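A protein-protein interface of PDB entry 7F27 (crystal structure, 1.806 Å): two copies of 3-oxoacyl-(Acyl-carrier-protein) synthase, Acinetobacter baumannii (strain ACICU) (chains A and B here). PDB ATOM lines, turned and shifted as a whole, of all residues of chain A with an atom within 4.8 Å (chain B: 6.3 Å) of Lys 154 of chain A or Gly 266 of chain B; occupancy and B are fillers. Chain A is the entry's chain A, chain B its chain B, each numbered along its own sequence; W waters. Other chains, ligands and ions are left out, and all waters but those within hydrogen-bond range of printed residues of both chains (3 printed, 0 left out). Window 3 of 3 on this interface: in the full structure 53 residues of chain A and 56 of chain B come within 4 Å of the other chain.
No position is printed for both chains.
Along chain A the printed residues that touch a printed residue of chain B span positions 148 to 156.
Of the 10 printed residues of chain B, 9 touch a printed residue of chain A.
Printed residues of chain B that touch a printed residue of chain A: Ser 262, Asn 263, Thr 264, Asp 265, Gly 266, Gln 267, His 268, Met 276 and Gly 395.
Hydrophobic or aromatic side chains of chain B that line the printed part of chain A: Met 276.
The backbone carbonyl oxygen (O) of Gly 396 of chain B lies within hydrogen-bond range of the backbone NH (N) of Asp 265 of chain B (2.8 Å).
The backbone NH (N) of Gly 155 of chain A is in hydrogen-bond range of the backbone carbonyl oxygen (O) of Ala 101 of chain A, 3.1 Å away.
ND2 of Asn 263 of chain B is in hydrogen-bond range of O of Met 276 of chain B.
The backbone carbonyl oxygen of Thr 148 of chain A is in hydrogen-bond range of the backbone NH of Leu 153 of chain A, 3.0 Å away.
Thr 148 of chain A touches Thr 264 of chain B (CB to CG2, 3.7 Å).
O of Thr 148 of chain A touches CA of Gly 266 of chain B, at 3.7 Å.
Thr 148 of chain A touches Gly 395 of chain B.
CG2 of Val 149 of chain A touches C of His 268 of chain B, 3.8 Å away.
Gly 152 of chain A touches Gly 266 of chain B.
Thr 264 of chain B touches Leu 153 of chain A (O to O, 3.8 Å).
Lys 154 of chain A touches Gly 266 of chain B.
Lys 154 of chain A touches Met 276 of chain B.
Gly 155 of chain A touches Asn 263 of chain B.
Leu 156 of chain A touches Thr 264 of chain B (C to OG1, 3.8 Å).
The backbone carbonyl oxygen of Gly 155 of chain A lies within hydrogen-bond range of the side-chain hydroxyl of Thr 264 of chain B, at 2.7 Å.
The side-chain amino group (NZ) of Lys 154 of chain A lies within hydrogen-bond range of the backbone carbonyl oxygen (O) of Asp 265 of chain B (3.3 Å).
The backbone carbonyl oxygen (O) of Lys 154 of chain A sits at hydrogen-bond distance from the backbone NH (N) of Thr 264 of chain B (3.4 Å).
Water W1 lies within hydrogen-bond range of the backbone carbonyl oxygen of Gly 395 of chain B, the side-chain hydroxyl of Thr 148 of chain A and the backbone NH of Gly 266 of chain B.
Water W3 bridges OG1 of Thr 148 of chain A and O of Gly 395 of chain B.
Water W2 bridges the backbone carbonyl oxygen of Lys 154 of chain A (2.8 Å) and the side-chain amide nitrogen of Asn 263 of chain B (3.2 Å).
Lys 154 of chain A touches five residues of chain B.
Of chain A, only Thr 148 (3.7 Å), Gly 152 (3.5 Å), Leu 153 (3.1 Å) and Lys 154 (3.8 Å) come within 4 Å of Gly 266 of chain B.
Of the printed residues of chain A, Asp 265 of chain B touches Lys 154.
Printed residues of chain A within 4 Å of Ser 262 of chain B: Leu 156 (3.5 Å).
Printed residues of chain A within 4 Å of His 268 of chain B: Val 149 (3.8 Å).
Gly 396 of chain B touches none of the printed residues of chain A.
Gly 99 of chain A touches none of the printed residues of chain B.
The nearest residue of chain B that does not touch Lys 154 of chain A is Gln 267 of chain B (4.6 Å).
The nearest printed residue of chain A that does not touch Asp 265 of chain B is Leu 153 of chain A (4.2 Å).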
ATOM      1  N   LEU A  96      14.349  11.340 -17.560  1.00  0.00           N
ATOM      2  CA  LEU A  96      13.170  10.483 -17.475  1.00  0.00           C
ATOM      3  C   LEU A  96      12.630  10.113 -18.853  1.00  0.00           C
ATOM      4  O   LEU A  96      12.123   8.998 -19.038  1.00  0.00           O
ATOM      5  CB  LEU A  96      12.089  11.169 -16.632  1.00  0.00           C
ATOM      6  CG  LEU A  96      12.337  11.304 -15.126  1.00  0.00           C
ATOM      7  CD1 LEU A  96      11.083  11.857 -14.449  1.00  0.00           C
ATOM      8  CD2 LEU A  96      12.779   9.967 -14.479  1.00  0.00           C
ATOM      9  N   SER A  97      12.740  11.012 -19.838  1.00  0.00           N
ATOM     10  CA  SER A  97      12.254  10.746 -21.188  1.00  0.00           C
ATOM     11  C   SER A  97      13.379  10.424 -22.170  1.00  0.00           C
ATOM     12  O   SER A  97      13.144  10.390 -23.386  1.00  0.00           O
ATOM     13  CB  SER A  97      11.425  11.931 -21.697  1.00  0.00           C
ATOM     14  OG  SER A  97      12.176  13.133 -21.638  1.00  0.00           O
ATOM     15  N   GLY A  99      15.080   7.571 -22.549  1.00  0.00           N
ATOM     16  CA  GLY A  99      15.299   6.162 -22.844  1.00  0.00           C
ATOM     17  C   GLY A  99      16.182   5.437 -21.843  1.00  0.00           C
ATOM     18  O   GLY A  99      16.222   4.198 -21.857  1.00  0.00           O
ATOM     19  N   ALA A 101      15.826   5.769 -18.520  1.00  0.00           N
ATOM     20  CA  ALA A 101      15.069   5.638 -17.284  1.00  0.00           C
ATOM     21  C   ALA A 101      13.879   4.723 -17.531  1.00  0.00           C
ATOM     22  O   ALA A 101      13.198   4.845 -18.557  1.00  0.00           O
ATOM     23  CB  ALA A 101      14.583   6.998 -16.776  1.00  0.00           C
ATOM     24  N   THR A 148       4.714   4.748 -16.855  1.00  0.00           N
ATOM     25  CA  THR A 148       5.449   5.134 -18.056  1.00  0.00           C
ATOM     26  C   THR A 148       4.700   6.208 -18.826  1.00  0.00           C
ATOM     27  O   THR A 148       5.319   7.111 -19.403  1.00  0.00           O
ATOM     28  CB  THR A 148       5.706   3.944 -18.983  1.00  0.00           C
ATOM     29  OG1 THR A 148       4.464   3.498 -19.530  1.00  0.00           O
ATOM     30  CG2 THR A 148       6.394   2.800 -18.253  1.00  0.00           C
ATOM     31  N   VAL A 149       3.371   6.125 -18.854  1.00  0.00           N
ATOM     32  CA  VAL A 149       2.592   7.120 -19.580  1.00  0.00           C
ATOM     33  C   VAL A 149       2.627   8.455 -18.842  1.00  0.00           C
ATOM     34  O   VAL A 149       2.902   9.500 -19.439  1.00  0.00           O
ATOM     35  CB  VAL A 149       1.155   6.618 -19.809  1.00  0.00           C
ATOM     36  CG1 VAL A 149       0.252   7.767 -20.230  1.00  0.00           C
ATOM     37  CG2 VAL A 149       1.138   5.495 -20.872  1.00  0.00           C
ATOM     38  N   GLY A 152       6.309   9.779 -18.817  1.00  0.00           N
ATOM     39  CA  GLY A 152       6.965   9.826 -20.114  1.00  0.00           C
ATOM     40  C   GLY A 152       8.199   8.958 -20.213  1.00  0.00           C
ATOM     41  O   GLY A 152       9.151   9.328 -20.912  1.00  0.00           O
ATOM     42  N   LEU A 153       8.212   7.815 -19.525  1.00  0.00           N
ATOM     43  CA  LEU A 153       9.383   6.944 -19.515  1.00  0.00           C
ATOM     44  C   LEU A 153       9.512   6.207 -20.835  1.00  0.00           C
ATOM     45  O   LEU A 153       8.530   5.682 -21.367  1.00  0.00           O
ATOM     46  CB  LEU A 153       9.282   5.935 -18.376  1.00  0.00           C
ATOM     47  CG  LEU A 153       9.007   6.498 -16.985  1.00  0.00           C
ATOM     48  CD1 LEU A 153       8.945   5.358 -15.973  1.00  0.00           C
ATOM     49  CD2 LEU A 153      10.076   7.505 -16.597  1.00  0.00           C
ATOM     50  N   LYS A 154      10.727   6.149 -21.366  1.00  0.00           N
ATOM     51  CA  LYS A 154      10.941   5.514 -22.658  1.00  0.00           C
ATOM     52  C   LYS A 154      11.924   4.358 -22.570  1.00  0.00           C
ATOM     53  O   LYS A 154      12.327   3.823 -23.611  1.00  0.00           O
ATOM     54  CB  LYS A 154      11.409   6.550 -23.685  1.00  0.00           C
ATOM     55  CG  LYS A 154      10.321   7.584 -24.040  1.00  0.00           C
ATOM     56  CD  LYS A 154      10.812   8.576 -25.084  1.00  0.00           C
ATOM     57  CE  LYS A 154       9.645   9.287 -25.761  1.00  0.00           C
ATOM     58  NZ  LYS A 154       8.575   9.587 -24.767  1.00  0.00           N
ATOM     59  N   GLY A 155      12.319   3.969 -21.357  1.00  0.00           N
ATOM     60  CA  GLY A 155      13.243   2.872 -21.155  1.00  0.00           C
ATOM     61  C   GLY A 155      12.504   1.569 -20.966  1.00  0.00           C
ATOM     62  O   GLY A 155      11.503   1.312 -21.642  1.00  0.00           O
ATOM     63  N   LEU A 156      12.972   0.754 -20.031  1.00  0.00           N
ATOM     64  CA  LEU A 156      12.402  -0.570 -19.809  1.00  0.00           C
ATOM     65  C   LEU A 156      11.117  -0.487 -19.000  1.00  0.00           C
ATOM     66  O   LEU A 156      11.052   0.226 -17.993  1.00  0.00           O
ATOM     67  CB  LEU A 156      13.384  -1.451 -19.048  1.00  0.00           C
ATOM     68  CG  LEU A 156      14.586  -2.023 -19.754  1.00  0.00           C
ATOM     69  CD1 LEU A 156      15.391  -2.767 -18.716  1.00  0.00           C
ATOM     70  CD2 LEU A 156      14.100  -2.952 -20.873  1.00  0.00           C
ATOM     71  N   SER B 262      14.128  -4.064 -25.760  1.00  0.00           N
ATOM     72  CA  SER B 262      12.824  -3.703 -25.225  1.00  0.00           C
ATOM     73  C   SER B 262      12.879  -2.249 -24.799  1.00  0.00           C
ATOM     74  O   SER B 262      13.866  -1.821 -24.200  1.00  0.00           O
ATOM     75  CB  SER B 262      12.420  -4.572 -24.024  1.00  0.00           C
ATOM     76  OG  SER B 262      11.063  -4.357 -23.670  1.00  0.00           O
ATOM     77  N   ASN B 263      11.821  -1.508 -25.102  1.00  0.00           N
ATOM     78  CA  ASN B 263      11.703  -0.125 -24.612  1.00  0.00           C
ATOM     79  C   ASN B 263      10.219   0.204 -24.515  1.00  0.00           C
ATOM     80  O   ASN B 263       9.368  -0.684 -24.599  1.00  0.00           O
ATOM     81  CB  ASN B 263      12.502   0.847 -25.486  1.00  0.00           C
ATOM     82  CG  ASN B 263      11.947   0.994 -26.885  1.00  0.00           C
ATOM     83  OD1 ASN B 263      10.904   0.438 -27.232  1.00  0.00           O
ATOM     84  ND2 ASN B 263      12.653   1.762 -27.706  1.00  0.00           N
ATOM     85  N   THR B 264       9.903   1.481 -24.328  1.00  0.00           N
ATOM     86  CA  THR B 264       8.548   1.874 -23.985  1.00  0.00           C
ATOM     87  C   THR B 264       8.222   3.187 -24.688  1.00  0.00           C
ATOM     88  O   THR B 264       9.069   4.075 -24.757  1.00  0.00           O
ATOM     89  CB  THR B 264       8.413   2.013 -22.463  1.00  0.00           C
ATOM     90  OG1 THR B 264       8.857   0.797 -21.833  1.00  0.00           O
ATOM     91  CG2 THR B 264       6.970   2.296 -22.059  1.00  0.00           C
ATOM     92  N   ASP B 265       7.001   3.299 -25.217  1.00  0.00           N
ATOM     93  CA  ASP B 265       6.640   4.491 -25.986  1.00  0.00           C
ATOM     94  C   ASP B 265       6.609   5.730 -25.097  1.00  0.00           C
ATOM     95  O   ASP B 265       7.042   6.811 -25.517  1.00  0.00           O
ATOM     96  CB  ASP B 265       5.280   4.305 -26.665  1.00  0.00           C
ATOM     97  CG  ASP B 265       5.347   3.405 -27.893  1.00  0.00           C
ATOM     98  OD1 ASP B 265       6.467   3.069 -28.336  1.00  0.00           O
ATOM     99  OD2 ASP B 265       4.270   3.027 -28.411  1.00  0.00           O
ATOM    100  N   GLY B 266       6.088   5.597 -23.878  1.00  0.00           N
ATOM    101  CA  GLY B 266       6.041   6.733 -22.963  1.00  0.00           C
ATOM    102  C   GLY B 266       5.074   7.823 -23.372  1.00  0.00           C
ATOM    103  O   GLY B 266       5.272   8.985 -23.006  1.00  0.00           O
ATOM    104  N   GLN B 267       4.019   7.477 -24.111  1.00  0.00           N
ATOM    105  CA  GLN B 267       3.127   8.470 -24.698  1.00  0.00           C
ATOM    106  C   GLN B 267       1.667   8.177 -24.390  1.00  0.00           C
ATOM    107  O   GLN B 267       0.947   9.044 -23.888  1.00  0.00           O
ATOM    108  CB  GLN B 267       3.325   8.530 -26.213  1.00  0.00           C
ATOM    109  CG  GLN B 267       4.417   9.483 -26.663  1.00  0.00           C
ATOM    110  CD  GLN B 267       3.860  10.831 -27.121  1.00  0.00           C
ATOM    111  OE1 GLN B 267       3.140  11.507 -26.376  1.00  0.00           O
ATOM    112  NE2 GLN B 267       4.180  11.219 -28.359  1.00  0.00           N
ATOM    113  N   HIS B 268       1.221   6.959 -24.682  1.00  0.00           N
ATOM    114  CA  HIS B 268      -0.199   6.641 -24.691  1.00  0.00           C
ATOM    115  C   HIS B 268      -0.402   5.168 -24.352  1.00  0.00           C
ATOM    116  O   HIS B 268       0.449   4.326 -24.654  1.00  0.00           O
ATOM    117  CB  HIS B 268      -0.818   6.952 -26.056  1.00  0.00           C
ATOM    118  CG  HIS B 268      -2.310   7.001 -26.034  1.00  0.00           C
ATOM    119  ND1 HIS B 268      -3.093   5.884 -26.242  1.00  0.00           N
ATOM    120  CD2 HIS B 268      -3.164   8.029 -25.815  1.00  0.00           C
ATOM    121  CE1 HIS B 268      -4.366   6.223 -26.153  1.00  0.00           C
ATOM    122  NE2 HIS B 268      -4.437   7.518 -25.893  1.00  0.00           N
ATOM    123  N   MET B 276       9.527   5.065 -31.378  1.00  0.00           N
ATOM    124  CA  MET B 276      10.044   4.214 -30.315  1.00  0.00           C
ATOM    125  C   MET B 276      10.043   2.745 -30.722  1.00  0.00           C
ATOM    126  O   MET B 276      10.944   2.003 -30.318  1.00  0.00           O
ATOM    127  CB  MET B 276       9.243   4.426 -29.032  1.00  0.00           C
ATOM    128  CG  MET B 276       9.367   5.847 -28.465  1.00  0.00           C
ATOM    129  SD  MET B 276      11.083   6.355 -28.254  1.00  0.00           S
ATOM    130  CE  MET B 276      11.643   5.158 -27.079  1.00  0.00           C
ATOM    131  N   GLY B 395       0.298   0.088 -23.336  1.00  0.00           N
ATOM    132  CA  GLY B 395       1.292   0.776 -22.553  1.00  0.00           C
ATOM    133  C   GLY B 395       2.537   1.096 -23.327  1.00  0.00           C
ATOM    134  O   GLY B 395       3.527   1.540 -22.729  1.00  0.00           O
ATOM    135  N   GLY B 396       2.523   0.858 -24.638  1.00  0.00           N
ATOM    136  CA  GLY B 396       3.670   1.138 -25.477  1.00  0.00           C
ATOM    137  C   GLY B 396       4.859   0.241 -25.221  1.00  0.00           C
ATOM    138  O   GLY B 396       5.995   0.663 -25.453  1.00  0.00           O
HETATM  139  O   HOH W   1       4.240   4.027 -22.318  1.00  0.00           O
HETATM  140  O   HOH W   2      14.158   3.798 -25.768  1.00  0.00           O
HETATM  141  O   HOH W   3       4.501   0.844 -20.128  1.00  0.00           O
